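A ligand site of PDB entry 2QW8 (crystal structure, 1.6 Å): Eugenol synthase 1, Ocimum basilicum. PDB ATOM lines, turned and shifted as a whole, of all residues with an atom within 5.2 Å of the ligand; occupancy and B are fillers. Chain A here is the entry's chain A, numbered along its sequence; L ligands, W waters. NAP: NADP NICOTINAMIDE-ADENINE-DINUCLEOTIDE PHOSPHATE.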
ATOM      1  N   GLY A  14      12.873 -13.342  10.003  1.00  0.00           N
ATOM      2  CA  GLY A  14      12.654 -14.733  10.330  1.00  0.00           C
ATOM      3  C   GLY A  14      13.589 -15.628   9.536  1.00  0.00           C
ATOM      4  O   GLY A  14      13.328 -16.812   9.359  1.00  0.00           O
ATOM      5  N   THR A  16      16.296 -16.982  10.307  1.00  0.00           N
ATOM      6  CA  THR A  16      16.891 -18.094  11.047  1.00  0.00           C
ATOM      7  C   THR A  16      15.856 -19.194  11.259  1.00  0.00           C
ATOM      8  O   THR A  16      16.156 -20.234  11.845  1.00  0.00           O
ATOM      9  CB  THR A  16      17.396 -17.658  12.447  1.00  0.00           C
ATOM     10  OG1 THR A  16      16.280 -17.184  13.222  1.00  0.00           O
ATOM     11  CG2 THR A  16      18.449 -16.560  12.315  1.00  0.00           C
ATOM     12  N   GLY A  17      14.648 -18.943  10.756  1.00  0.00           N
ATOM     13  CA  GLY A  17      13.546 -19.883  10.921  1.00  0.00           C
ATOM     14  C   GLY A  17      13.612 -21.202  10.175  1.00  0.00           C
ATOM     15  O   GLY A  17      14.490 -21.445   9.354  1.00  0.00           O
ATOM     16  N   TYR A  18      12.635 -22.054  10.450  1.00  0.00           N
ATOM     17  CA  TYR A  18      12.570 -23.360   9.822  1.00  0.00           C
ATOM     18  C   TYR A  18      12.559 -23.248   8.309  1.00  0.00           C
ATOM     19  O   TYR A  18      13.316 -23.950   7.627  1.00  0.00           O
ATOM     20  CB  TYR A  18      11.332 -24.124  10.303  1.00  0.00           C
ATOM     21  CG  TYR A  18      11.273 -25.509   9.725  1.00  0.00           C
ATOM     22  CD1 TYR A  18      12.099 -26.524  10.206  1.00  0.00           C
ATOM     23  CD2 TYR A  18      10.442 -25.802   8.648  1.00  0.00           C
ATOM     24  CE1 TYR A  18      12.097 -27.798   9.626  1.00  0.00           C
ATOM     25  CE2 TYR A  18      10.428 -27.059   8.061  1.00  0.00           C
ATOM     26  CZ  TYR A  18      11.254 -28.054   8.562  1.00  0.00           C
ATOM     27  OH  TYR A  18      11.223 -29.307   7.972  1.00  0.00           O
ATOM     28  N   ILE A  19      11.713 -22.378   7.764  1.00  0.00           N
ATOM     29  CA  ILE A  19      11.684 -22.216   6.311  1.00  0.00           C
ATOM     30  C   ILE A  19      12.535 -21.009   5.916  1.00  0.00           C
ATOM     31  O   ILE A  19      13.090 -20.955   4.808  1.00  0.00           O
ATOM     32  CB  ILE A  19      10.224 -22.027   5.783  1.00  0.00           C
ATOM     33  CG1 ILE A  19      10.188 -22.257   4.261  1.00  0.00           C
ATOM     34  CG2 ILE A  19       9.702 -20.643   6.125  1.00  0.00           C
ATOM     35  CD1 ILE A  19      10.472 -23.709   3.852  1.00  0.00           C
ATOM     36  N   GLY A  20      12.648 -20.044   6.819  1.00  0.00           N
ATOM     37  CA  GLY A  20      13.433 -18.858   6.537  1.00  0.00           C
ATOM     38  C   GLY A  20      14.890 -19.116   6.188  1.00  0.00           C
ATOM     39  O   GLY A  20      15.443 -18.453   5.313  1.00  0.00           O
ATOM     40  N   PHE A  37      17.454 -10.182   9.368  1.00  0.00           N
ATOM     41  CA  PHE A  37      17.086  -9.490  10.599  1.00  0.00           C
ATOM     42  C   PHE A  37      16.850 -10.561  11.664  1.00  0.00           C
ATOM     43  O   PHE A  37      16.103 -11.512  11.434  1.00  0.00           O
ATOM     44  CB  PHE A  37      15.820  -8.661  10.381  1.00  0.00           C
ATOM     45  CG  PHE A  37      15.589  -7.619  11.443  1.00  0.00           C
ATOM     46  CD1 PHE A  37      16.278  -6.405  11.412  1.00  0.00           C
ATOM     47  CD2 PHE A  37      14.689  -7.840  12.475  1.00  0.00           C
ATOM     48  CE1 PHE A  37      16.060  -5.439  12.391  1.00  0.00           C
ATOM     49  CE2 PHE A  37      14.467  -6.888  13.456  1.00  0.00           C
ATOM     50  CZ  PHE A  37      15.156  -5.684  13.416  1.00  0.00           C
ATOM     51  N   THR A  38      17.492 -10.406  12.821  1.00  0.00           N
ATOM     52  CA  THR A  38      17.349 -11.381  13.897  1.00  0.00           C
ATOM     53  C   THR A  38      17.362 -10.699  15.261  1.00  0.00           C
ATOM     54  O   THR A  38      17.966  -9.639  15.425  1.00  0.00           O
ATOM     55  CB  THR A  38      18.509 -12.417  13.816  1.00  0.00           C
ATOM     56  OG1 THR A  38      18.397 -13.354  14.903  1.00  0.00           O
ATOM     57  CG2 THR A  38      19.856 -11.720  13.877  1.00  0.00           C
ATOM     58  N   ARG A  39      16.686 -11.291  16.248  1.00  0.00           N
ATOM     59  CA  ARG A  39      16.639 -10.733  17.587  1.00  0.00           C
ATOM     60  C   ARG A  39      18.008 -10.794  18.257  1.00  0.00           C
ATOM     61  O   ARG A  39      18.823 -11.660  17.965  1.00  0.00           O
ATOM     62  CB  ARG A  39      15.632 -11.501  18.455  1.00  0.00           C
ATOM     63  CG  ARG A  39      14.178 -11.276  18.051  1.00  0.00           C
ATOM     64  CD  ARG A  39      13.273 -12.259  18.772  1.00  0.00           C
ATOM     65  NE  ARG A  39      13.602 -13.639  18.430  1.00  0.00           N
ATOM     66  CZ  ARG A  39      13.215 -14.691  19.149  1.00  0.00           C
ATOM     67  NH1 ARG A  39      13.562 -15.918  18.775  1.00  0.00           N
ATOM     68  NH2 ARG A  39      12.497 -14.509  20.256  1.00  0.00           N
ATOM     69  N   SER A  42      18.420 -14.204  20.150  1.00  0.00           N
ATOM     70  CA  SER A  42      18.214 -15.457  19.444  1.00  0.00           C
ATOM     71  C   SER A  42      19.319 -16.483  19.712  1.00  0.00           C
ATOM     72  O   SER A  42      20.501 -16.134  19.792  1.00  0.00           O
ATOM     73  CB  SER A  42      18.118 -15.222  17.930  1.00  0.00           C
ATOM     74  OG  SER A  42      17.973 -16.447  17.225  1.00  0.00           O
ATOM     75  N   SER A  43      18.921 -17.744  19.834  1.00  0.00           N
ATOM     76  CA  SER A  43      19.871 -18.829  20.082  1.00  0.00           C
ATOM     77  C   SER A  43      20.448 -19.385  18.792  1.00  0.00           C
ATOM     78  O   SER A  43      21.267 -20.304  18.819  1.00  0.00           O
ATOM     79  CB  SER A  43      19.180 -19.950  20.867  1.00  0.00           C
ATOM     80  OG  SER A  43      18.082 -20.479  20.147  1.00  0.00           O
ATOM     81  N   LYS A  44      20.037 -18.821  17.665  1.00  0.00           N
ATOM     82  CA  LYS A  44      20.502 -19.260  16.349  1.00  0.00           C
ATOM     83  C   LYS A  44      21.900 -18.692  16.030  1.00  0.00           C
ATOM     84  O   LYS A  44      22.176 -18.349  14.879  1.00  0.00           O
ATOM     85  CB  LYS A  44      19.513 -18.780  15.277  1.00  0.00           C
ATOM     86  CG  LYS A  44      18.058 -19.199  15.489  1.00  0.00           C
ATOM     87  CD  LYS A  44      17.857 -20.695  15.252  1.00  0.00           C
ATOM     88  CE  LYS A  44      16.388 -21.069  15.412  1.00  0.00           C
ATOM     89  NZ  LYS A  44      15.515 -20.413  14.392  1.00  0.00           N
ATOM     90  N   LEU A  63      11.522  -5.955  16.270  1.00  0.00           N
ATOM     91  CA  LEU A  63      10.547  -5.413  15.345  1.00  0.00           C
ATOM     92  C   LEU A  63       9.971  -4.089  15.846  1.00  0.00           C
ATOM     93  O   LEU A  63       9.422  -3.312  15.058  1.00  0.00           O
ATOM     94  CB  LEU A  63       9.415  -6.424  15.123  1.00  0.00           C
ATOM     95  CG  LEU A  63       9.828  -7.708  14.406  1.00  0.00           C
ATOM     96  CD1 LEU A  63       8.640  -8.645  14.300  1.00  0.00           C
ATOM     97  CD2 LEU A  63      10.354  -7.375  13.012  1.00  0.00           C
ATOM     98  N   ALA A  82       9.342 -14.442   6.951  1.00  0.00           N
ATOM     99  CA  ALA A  82       9.146 -15.861   7.224  1.00  0.00           C
ATOM    100  C   ALA A  82       8.888 -16.020   8.720  1.00  0.00           C
ATOM    101  O   ALA A  82       9.333 -16.983   9.335  1.00  0.00           O
ATOM    102  CB  ALA A  82      10.386 -16.651   6.819  1.00  0.00           C
ATOM    103  N   LEU A  83       8.172 -15.058   9.304  1.00  0.00           N
ATOM    104  CA  LEU A  83       7.829 -15.084  10.719  1.00  0.00           C
ATOM    105  C   LEU A  83       6.790 -16.168  11.024  1.00  0.00           C
ATOM    106  O   LEU A  83       6.042 -16.595  10.148  1.00  0.00           O
ATOM    107  CB  LEU A  83       7.319 -13.709  11.168  1.00  0.00           C
ATOM    108  CG  LEU A  83       8.353 -12.580  11.106  1.00  0.00           C
ATOM    109  CD1 LEU A  83       7.748 -11.301  11.663  1.00  0.00           C
ATOM    110  CD2 LEU A  83       9.582 -12.973  11.919  1.00  0.00           C
ATOM    111  N   ALA A  84       6.744 -16.597  12.285  1.00  0.00           N
ATOM    112  CA  ALA A  84       5.834 -17.646  12.733  1.00  0.00           C
ATOM    113  C   ALA A  84       4.434 -17.169  13.084  1.00  0.00           C
ATOM    114  O   ALA A  84       4.189 -15.974  13.230  1.00  0.00           O
ATOM    115  CB  ALA A  84       6.445 -18.370  13.935  1.00  0.00           C
ATOM    116  N   PHE A  85       3.512 -18.116  13.222  1.00  0.00           N
ATOM    117  CA  PHE A  85       2.127 -17.800  13.553  1.00  0.00           C
ATOM    118  C   PHE A  85       1.908 -16.785  14.672  1.00  0.00           C
ATOM    119  O   PHE A  85       1.084 -15.882  14.541  1.00  0.00           O
ATOM    120  CB  PHE A  85       1.367 -19.087  13.915  1.00  0.00           C
ATOM    121  CG  PHE A  85       0.819 -19.842  12.733  1.00  0.00           C
ATOM    122  CD1 PHE A  85       0.953 -21.227  12.638  1.00  0.00           C
ATOM    123  CD2 PHE A  85       0.163 -19.167  11.710  1.00  0.00           C
ATOM    124  CE1 PHE A  85       0.435 -21.924  11.547  1.00  0.00           C
ATOM    125  CE2 PHE A  85      -0.365 -19.854  10.619  1.00  0.00           C
ATOM    126  CZ  PHE A  85      -0.230 -21.229  10.534  1.00  0.00           C
ATOM    127  N   GLN A  87       3.615 -14.323  15.456  1.00  0.00           N
ATOM    128  CA  GLN A  87       4.041 -13.001  15.026  1.00  0.00           C
ATOM    129  C   GLN A  87       3.383 -12.494  13.742  1.00  0.00           C
ATOM    130  O   GLN A  87       3.859 -11.533  13.130  1.00  0.00           O
ATOM    131  CB  GLN A  87       5.568 -12.999  14.836  1.00  0.00           C
ATOM    132  CG  GLN A  87       6.408 -12.938  16.122  1.00  0.00           C
ATOM    133  CD  GLN A  87       6.312 -14.200  16.974  1.00  0.00           C
ATOM    134  OE1 GLN A  87       6.661 -15.300  16.534  1.00  0.00           O
ATOM    135  NE2 GLN A  87       5.846 -14.044  18.212  1.00  0.00           N
ATOM    136  N   ILE A  88       2.281 -13.112  13.339  1.00  0.00           N
ATOM    137  CA  ILE A  88       1.639 -12.706  12.094  1.00  0.00           C
ATOM    138  C   ILE A  88       1.240 -11.231  12.056  1.00  0.00           C
ATOM    139  O   ILE A  88       1.565 -10.530  11.097  1.00  0.00           O
ATOM    140  CB  ILE A  88       0.407 -13.569  11.768  1.00  0.00           C
ATOM    141  CG1 ILE A  88       0.865 -15.011  11.545  1.00  0.00           C
ATOM    142  CG2 ILE A  88      -0.300 -13.031  10.523  1.00  0.00           C
ATOM    143  CD1 ILE A  88       1.956 -15.163  10.480  1.00  0.00           C
ATOM    144  N   SER A 110       4.451 -13.529   5.305  1.00  0.00           N
ATOM    145  CA  SER A 110       4.611 -14.904   5.747  1.00  0.00           C
ATOM    146  C   SER A 110       3.374 -15.761   5.534  1.00  0.00           C
ATOM    147  O   SER A 110       2.573 -15.939   6.462  1.00  0.00           O
ATOM    148  CB  SER A 110       5.011 -14.942   7.220  1.00  0.00           C
ATOM    149  OG  SER A 110       5.401 -16.249   7.599  1.00  0.00           O
ATOM    150  N   ASP A 111       3.214 -16.279   4.329  1.00  0.00           N
ATOM    151  CA  ASP A 111       2.094 -17.163   4.021  1.00  0.00           C
ATOM    152  C   ASP A 111       2.726 -18.566   4.014  1.00  0.00           C
ATOM    153  O   ASP A 111       2.744 -19.256   5.024  1.00  0.00           O
ATOM    154  CB  ASP A 111       1.466 -16.804   2.664  1.00  0.00           C
ATOM    155  CG  ASP A 111       0.665 -15.510   2.711  1.00  0.00           C
ATOM    156  OD1 ASP A 111      -0.014 -15.245   3.736  1.00  0.00           O
ATOM    157  OD2 ASP A 111       0.689 -14.751   1.722  1.00  0.00           O
ATOM    158  N   PHE A 112       3.274 -18.965   2.867  1.00  0.00           N
ATOM    159  CA  PHE A 112       3.952 -20.248   2.721  1.00  0.00           C
ATOM    160  C   PHE A 112       3.193 -21.466   3.213  1.00  0.00           C
ATOM    161  O   PHE A 112       3.747 -22.335   3.874  1.00  0.00           O
ATOM    162  CB  PHE A 112       5.332 -20.172   3.405  1.00  0.00           C
ATOM    163  CG  PHE A 112       6.153 -19.014   2.930  1.00  0.00           C
ATOM    164  CD1 PHE A 112       6.404 -17.930   3.772  1.00  0.00           C
ATOM    165  CD2 PHE A 112       6.595 -18.961   1.617  1.00  0.00           C
ATOM    166  CE1 PHE A 112       7.081 -16.789   3.298  1.00  0.00           C
ATOM    167  CE2 PHE A 112       7.264 -17.838   1.129  1.00  0.00           C
ATOM    168  CZ  PHE A 112       7.509 -16.760   1.968  1.00  0.00           C
ATOM    169  N   GLY A 113       1.915 -21.530   2.854  1.00  0.00           N
ATOM    170  CA  GLY A 113       1.120 -22.666   3.266  1.00  0.00           C
ATOM    171  C   GLY A 113      -0.052 -22.811   2.328  1.00  0.00           C
ATOM    172  O   GLY A 113       0.114 -22.860   1.110  1.00  0.00           O
ATOM    173  N   LYS A 132      -3.423 -13.808   8.546  1.00  0.00           N
ATOM    174  CA  LYS A 132      -2.623 -13.692   7.331  1.00  0.00           C
ATOM    175  C   LYS A 132      -3.425 -12.921   6.276  1.00  0.00           C
ATOM    176  O   LYS A 132      -2.867 -12.156   5.488  1.00  0.00           O
ATOM    177  CB  LYS A 132      -2.209 -15.071   6.817  1.00  0.00           C
ATOM    178  CG  LYS A 132      -1.308 -15.797   7.797  1.00  0.00           C
ATOM    179  CD  LYS A 132      -0.712 -17.055   7.190  1.00  0.00           C
ATOM    180  CE  LYS A 132       0.408 -17.598   8.064  1.00  0.00           C
ATOM    181  NZ  LYS A 132       1.053 -18.791   7.441  1.00  0.00           N
ATOM    182  N   ASN A 152       2.142 -24.770  -0.103  1.00  0.00           N
ATOM    183  CA  ASN A 152       1.526 -26.039   0.258  1.00  0.00           C
ATOM    184  C   ASN A 152       2.303 -26.705   1.400  1.00  0.00           C
ATOM    185  O   ASN A 152       2.926 -26.000   2.183  1.00  0.00           O
ATOM    186  CB  ASN A 152       1.390 -26.931  -0.965  1.00  0.00           C
ATOM    187  CG  ASN A 152       0.293 -26.445  -1.892  1.00  0.00           C
ATOM    188  OD1 ASN A 152      -0.784 -26.044  -1.433  1.00  0.00           O
ATOM    189  ND2 ASN A 152       0.545 -26.473  -3.202  1.00  0.00           N
ATOM    190  N   CYS A 153       2.286 -28.026   1.513  1.00  0.00           N
ATOM    191  CA  CYS A 153       2.951 -28.692   2.647  1.00  0.00           C
ATOM    192  C   CYS A 153       4.476 -28.767   2.603  1.00  0.00           C
ATOM    193  O   CYS A 153       5.051 -29.101   1.570  1.00  0.00           O
ATOM    194  CB  CYS A 153       2.422 -30.122   2.819  1.00  0.00           C
ATOM    195  SG  CYS A 153       0.621 -30.245   2.994  1.00  0.00           S
ATOM    196  N   PHE A 154       5.130 -28.465   3.724  1.00  0.00           N
ATOM    197  CA  PHE A 154       6.591 -28.552   3.803  1.00  0.00           C
ATOM    198  C   PHE A 154       6.842 -30.059   3.845  1.00  0.00           C
ATOM    199  O   PHE A 154       6.435 -30.730   4.796  1.00  0.00           O
ATOM    200  CB  PHE A 154       7.132 -27.881   5.067  1.00  0.00           C
ATOM    201  CG  PHE A 154       7.111 -26.372   5.028  1.00  0.00           C
ATOM    202  CD1 PHE A 154       6.590 -25.678   3.933  1.00  0.00           C
ATOM    203  CD2 PHE A 154       7.597 -25.638   6.112  1.00  0.00           C
ATOM    204  CE1 PHE A 154       6.562 -24.273   3.927  1.00  0.00           C
ATOM    205  CE2 PHE A 154       7.571 -24.239   6.112  1.00  0.00           C
ATOM    206  CZ  PHE A 154       7.051 -23.555   5.008  1.00  0.00           C
ATOM    207  N   TYR A 157       9.046 -31.728   6.797  1.00  0.00           N
ATOM    208  CA  TYR A 157       8.232 -31.510   7.970  1.00  0.00           C
ATOM    209  C   TYR A 157       7.137 -32.560   8.095  1.00  0.00           C
ATOM    210  O   TYR A 157       7.012 -33.219   9.126  1.00  0.00           O
ATOM    211  CB  TYR A 157       7.597 -30.120   7.920  1.00  0.00           C
ATOM    212  CG  TYR A 157       6.898 -29.716   9.185  1.00  0.00           C
ATOM    213  CD1 TYR A 157       7.502 -28.835  10.082  1.00  0.00           C
ATOM    214  CD2 TYR A 157       5.629 -30.202   9.501  1.00  0.00           C
ATOM    215  CE1 TYR A 157       6.863 -28.452  11.268  1.00  0.00           C
ATOM    216  CE2 TYR A 157       4.984 -29.836  10.673  1.00  0.00           C
ATOM    217  CZ  TYR A 157       5.614 -28.958  11.553  1.00  0.00           C
ATOM    218  OH  TYR A 157       4.970 -28.572  12.716  1.00  0.00           O
ATOM    219  N   PHE A 158       6.347 -32.718   7.032  1.00  0.00           N
ATOM    220  CA  PHE A 158       5.262 -33.681   7.091  1.00  0.00           C
ATOM    221  C   PHE A 158       5.607 -35.133   6.819  1.00  0.00           C
ATOM    222  O   PHE A 158       4.857 -36.013   7.217  1.00  0.00           O
ATOM    223  CB  PHE A 158       4.087 -33.210   6.229  1.00  0.00           C
ATOM    224  CG  PHE A 158       3.298 -32.112   6.879  1.00  0.00           C
ATOM    225  CD1 PHE A 158       3.472 -30.782   6.495  1.00  0.00           C
ATOM    226  CD2 PHE A 158       2.438 -32.392   7.938  1.00  0.00           C
ATOM    227  CE1 PHE A 158       2.804 -29.756   7.153  1.00  0.00           C
ATOM    228  CE2 PHE A 158       1.766 -31.369   8.610  1.00  0.00           C
ATOM    229  CZ  PHE A 158       1.944 -30.056   8.222  1.00  0.00           C
ATOM    230  N   ALA A 312       6.155 -26.715  14.466  1.00  0.00           N
ATOM    231  CA  ALA A 312       5.845 -25.293  14.349  1.00  0.00           C
ATOM    232  C   ALA A 312       5.430 -24.662  15.672  1.00  0.00           C
ATOM    233  O   ALA A 312       4.913 -25.340  16.561  1.00  0.00           O
ATOM    234  CB  ALA A 312       4.747 -25.089  13.313  1.00  0.00           C
ATOM    235  N   ALA A 313       5.663 -23.350  15.783  1.00  0.00           N
ATOM    236  CA  ALA A 313       5.304 -22.610  16.998  1.00  0.00           C
ATOM    237  C   ALA A 313       3.875 -22.098  16.905  1.00  0.00           C
ATOM    238  O   ALA A 313       3.458 -21.577  15.871  1.00  0.00           O
ATOM    239  CB  ALA A 313       6.255 -21.440  17.194  1.00  0.00           C
HETATM  240  PA  NAP L   1       9.851 -20.393  13.036  1.00  0.00           P
HETATM  241  O1A NAP L   1       9.061 -20.849  14.199  1.00  0.00           O
HETATM  242  O2A NAP L   1      11.053 -21.132  12.611  1.00  0.00           O
HETATM  243  O5B NAP L   1      10.169 -18.864  13.359  1.00  0.00           O
HETATM  244  C5B NAP L   1      10.795 -18.056  12.359  1.00  0.00           C
HETATM  245  C4B NAP L   1      11.578 -17.010  13.089  1.00  0.00           C
HETATM  246  O4B NAP L   1      10.808 -16.018  13.953  1.00  0.00           O
HETATM  247  C3B NAP L   1      12.516 -17.458  14.201  1.00  0.00           C
HETATM  248  O3B NAP L   1      13.656 -18.111  13.652  1.00  0.00           O
HETATM  249  C2B NAP L   1      12.881 -16.191  15.000  1.00  0.00           C
HETATM  250  O2B NAP L   1      14.057 -15.601  14.474  1.00  0.00           O
HETATM  251  C1B NAP L   1      11.671 -15.281  14.809  1.00  0.00           C
HETATM  252  N9A NAP L   1      10.934 -15.030  16.056  1.00  0.00           N
HETATM  253  C8A NAP L   1      10.531 -15.978  16.992  1.00  0.00           C
HETATM  254  N7A NAP L   1       9.886 -15.458  18.022  1.00  0.00           N
HETATM  255  C5A NAP L   1       9.872 -14.129  17.752  1.00  0.00           C
HETATM  256  C6A NAP L   1       9.336 -13.027  18.473  1.00  0.00           C
HETATM  257  N6A NAP L   1       8.709 -13.195  19.646  1.00  0.00           N
HETATM  258  N1A NAP L   1       9.487 -11.768  17.921  1.00  0.00           N
HETATM  259  C2A NAP L   1      10.127 -11.607  16.735  1.00  0.00           C
HETATM  260  N3A NAP L   1      10.679 -12.589  15.965  1.00  0.00           N
HETATM  261  C4A NAP L   1      10.508 -13.827  16.546  1.00  0.00           C
HETATM  262  O3  NAP L   1       8.816 -20.180  11.802  1.00  0.00           O
HETATM  263  PN  NAP L   1       8.421 -21.295  10.724  1.00  0.00           P
HETATM  264  O1N NAP L   1       8.066 -22.597  11.382  1.00  0.00           O
HETATM  265  O2N NAP L   1       9.532 -21.321   9.733  1.00  0.00           O
HETATM  266  O5D NAP L   1       7.146 -20.664   9.994  1.00  0.00           O
HETATM  267  C5D NAP L   1       7.267 -19.582   9.051  1.00  0.00           C
HETATM  268  C4D NAP L   1       6.086 -19.600   8.097  1.00  0.00           C
HETATM  269  O4D NAP L   1       6.007 -20.908   7.472  1.00  0.00           O
HETATM  270  C3D NAP L   1       4.723 -19.270   8.761  1.00  0.00           C
HETATM  271  O3D NAP L   1       3.940 -18.422   7.957  1.00  0.00           O
HETATM  272  C2D NAP L   1       4.173 -20.653   8.946  1.00  0.00           C
HETATM  273  O2D NAP L   1       2.756 -20.592   9.032  1.00  0.00           O
HETATM  274  C1D NAP L   1       4.685 -21.415   7.760  1.00  0.00           C
HETATM  275  N1N NAP L   1       4.675 -22.873   7.969  1.00  0.00           N
HETATM  276  C2N NAP L   1       4.120 -23.632   6.950  1.00  0.00           C
HETATM  277  C3N NAP L   1       4.266 -25.025   6.962  1.00  0.00           C
HETATM  278  C7N NAP L   1       3.767 -25.869   5.817  1.00  0.00           C
HETATM  279  O7N NAP L   1       3.814 -27.092   5.912  1.00  0.00           O
HETATM  280  N7N NAP L   1       3.335 -25.238   4.723  1.00  0.00           N
HETATM  281  C4N NAP L   1       4.898 -25.663   8.079  1.00  0.00           C
HETATM  282  C5N NAP L   1       5.454 -24.864   9.108  1.00  0.00           C
HETATM  283  C6N NAP L   1       5.369 -23.473   9.037  1.00  0.00           C
HETATM  284  P2B NAP L   1      15.232 -14.969  15.398  1.00  0.00           P
HETATM  285  O1X NAP L   1      15.493 -15.935  16.527  1.00  0.00           O
HETATM  286  O2X NAP L   1      16.346 -14.818  14.392  1.00  0.00           O
HETATM  287  O3X NAP L   1      14.717 -13.627  15.890  1.00  0.00           O
HETATM  288  O   HOH W   1       9.966 -23.126  15.618  1.00  0.00           O
HETATM  289  O   HOH W   2       6.655 -22.008  13.620  1.00  0.00           O
HETATM  290  O   HOH W   3      12.901 -22.081  14.271  1.00  0.00           O
HETATM  291  O   HOH W   4       3.246 -22.726  11.292  1.00  0.00           O
HETATM  292  O   HOH W   5      11.500  -8.636  17.410  1.00  0.00           O
HETATM  293  O   HOH W   6      10.989 -19.269   9.089  1.00  0.00           O
HETATM  294  O   HOH W   7       8.188 -25.236  11.901  1.00  0.00           O
HETATM  295  O   HOH W   8      15.731 -14.256  11.769  1.00  0.00           O
HETATM  296  O   HOH W   9       8.108 -15.257  14.266  1.00  0.00           O
HETATM  297  O   HOH W  10       9.304 -19.266  16.558  1.00  0.00           O
HETATM  298  O   HOH W  11      13.232 -11.834  14.493  1.00  0.00           O
HETATM  299  O   HOH W  12      15.044 -18.558  16.644  1.00  0.00           O
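The side-chain hydroxyl (OG) of Ser 42 lies within hydrogen-bond range of the backbone NH (N) of Lys 44.
The backbone carbonyl oxygen (O) of Thr 16 lies within hydrogen-bond range of the side-chain amino group (NZ) of Lys 44 (2.6 Å).
The backbone carbonyl oxygen of Ser 110 lies close to the side-chain amino group of Lys 132.
The backbone carbonyl oxygen (O) of Leu 83 is in hydrogen-bond range of the side-chain hydroxyl (OG) of Ser 110 (2.7 Å).
The backbone NH of Asn 152 is in hydrogen-bond range of the backbone carbonyl oxygen of Gly 113, 3.0 Å away.
OH of Tyr 18 lies within hydrogen-bond range of N of Tyr 157 (3.5 Å).
The side-chain amino group (NZ) of Lys 132 sits at hydrogen-bond distance from the backbone carbonyl oxygen (O) of Asp 111 (3.0 Å).
Water W6 lies within hydrogen-bond range of O2N of the ligand (2.6 Å), O of Ala 82 (2.8 Å), N of Gly 20 (2.9 Å), O of Gly 14 (3.4 Å) and N of Ile 19 (3.5 Å).
Water W3 lies within hydrogen-bond range of O2A of the ligand (2.7 Å) and NZ of Lys 44 (3.1 Å).
Water W12 lies within hydrogen-bond range of O1X of the ligand (2.7 Å) and NZ of Lys 44 (3.0 Å).
Water W2 lies within hydrogen-bond range of an oxygen (O1N) of the ligand (2.7 Å) and the backbone NH (N) of Ala 313 (2.7 Å).
Water W8 lies within hydrogen-bond range of an oxygen (O2X) of the ligand (2.8 Å), the backbone carbonyl oxygen of Phe 37 (2.8 Å), the backbone NH of Thr 16 (3.1 Å) and the backbone NH of Gly 14 (3.5 Å).
Water W9 lies within hydrogen-bond range of OE1 of Gln 87 (2.7 Å), N of Ala 84 (2.8 Å) and O4B of the ligand (2.8 Å).
OG1 of Thr 38 sits at hydrogen-bond distance from O2X of the ligand (2.6 Å).
An oxygen (O1X) of the ligand lies within hydrogen-bond range of the side-chain hydroxyl (OG) of Ser 42 (2.6 Å).
An oxygen (O2X) of the ligand sits at hydrogen-bond distance from the side-chain hydroxyl (OG1) of Thr 16 (2.6 Å).
An oxygen (O3D) of the ligand lies within hydrogen-bond range of the backbone carbonyl oxygen (O) of Ser 110 (3.2 Å).
O3D of the ligand lies within hydrogen-bond range of OG of Ser 110, 2.6 Å away.
A nitrogen (N7N) of the ligand lies within hydrogen-bond range of the backbone carbonyl oxygen (O) of Asn 152, 2.7 Å away.
N of Arg 39 sits at hydrogen-bond distance from O3X of the ligand (3.1 Å).
The guanidinium group (NE) of Arg 39 is in salt-bridge range of an oxygen (O3X) of the ligand, 2.8 Å away.
O2A of the ligand is in hydrogen-bond range of N of Tyr 18 (2.8 Å).
The backbone NH (N) of Phe 154 lies within hydrogen-bond range of an oxygen (O7N) of the ligand (2.9 Å).
An oxygen (O2D) of the ligand sits at hydrogen-bond distance from the side-chain amino group of Lys 132.
NZ of Lys 44 sits at hydrogen-bond distance from O3B of the ligand, 3.1 Å away.
O of Phe 112 lies within hydrogen-bond range of N7N of the ligand (3.1 Å).
The backbone NH of Ile 19 is in hydrogen-bond range of an oxygen (O2N) of the ligand, 3.1 Å away.
The backbone NH (N) of Gly 17 lies within hydrogen-bond range of an oxygen (O3B) of the ligand, at 3.2 Å.
O of Asp 111 sits at hydrogen-bond distance from O3D of the ligand (3.3 Å).
N6A of the ligand lies close to NE2 of Gln 87 (3.3 Å).
Residues that only touch the ligand: Gly 14, Ala 82, Leu 83, Ala 84, Phe 85, Gly 113, Cys 153 and Phe 158.
Hydrophobic or aromatic side chains within 4 Å of the ligand: Tyr 18, Ile 19, Leu 83, Ala 84, Phe 85, Phe 154 and Phe 158.
Of the 31 residues printed, 23 come within 4 Å of the ligand.
The nearest printed residue that does not touch the ligand is Leu 63 (4.1 Å).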
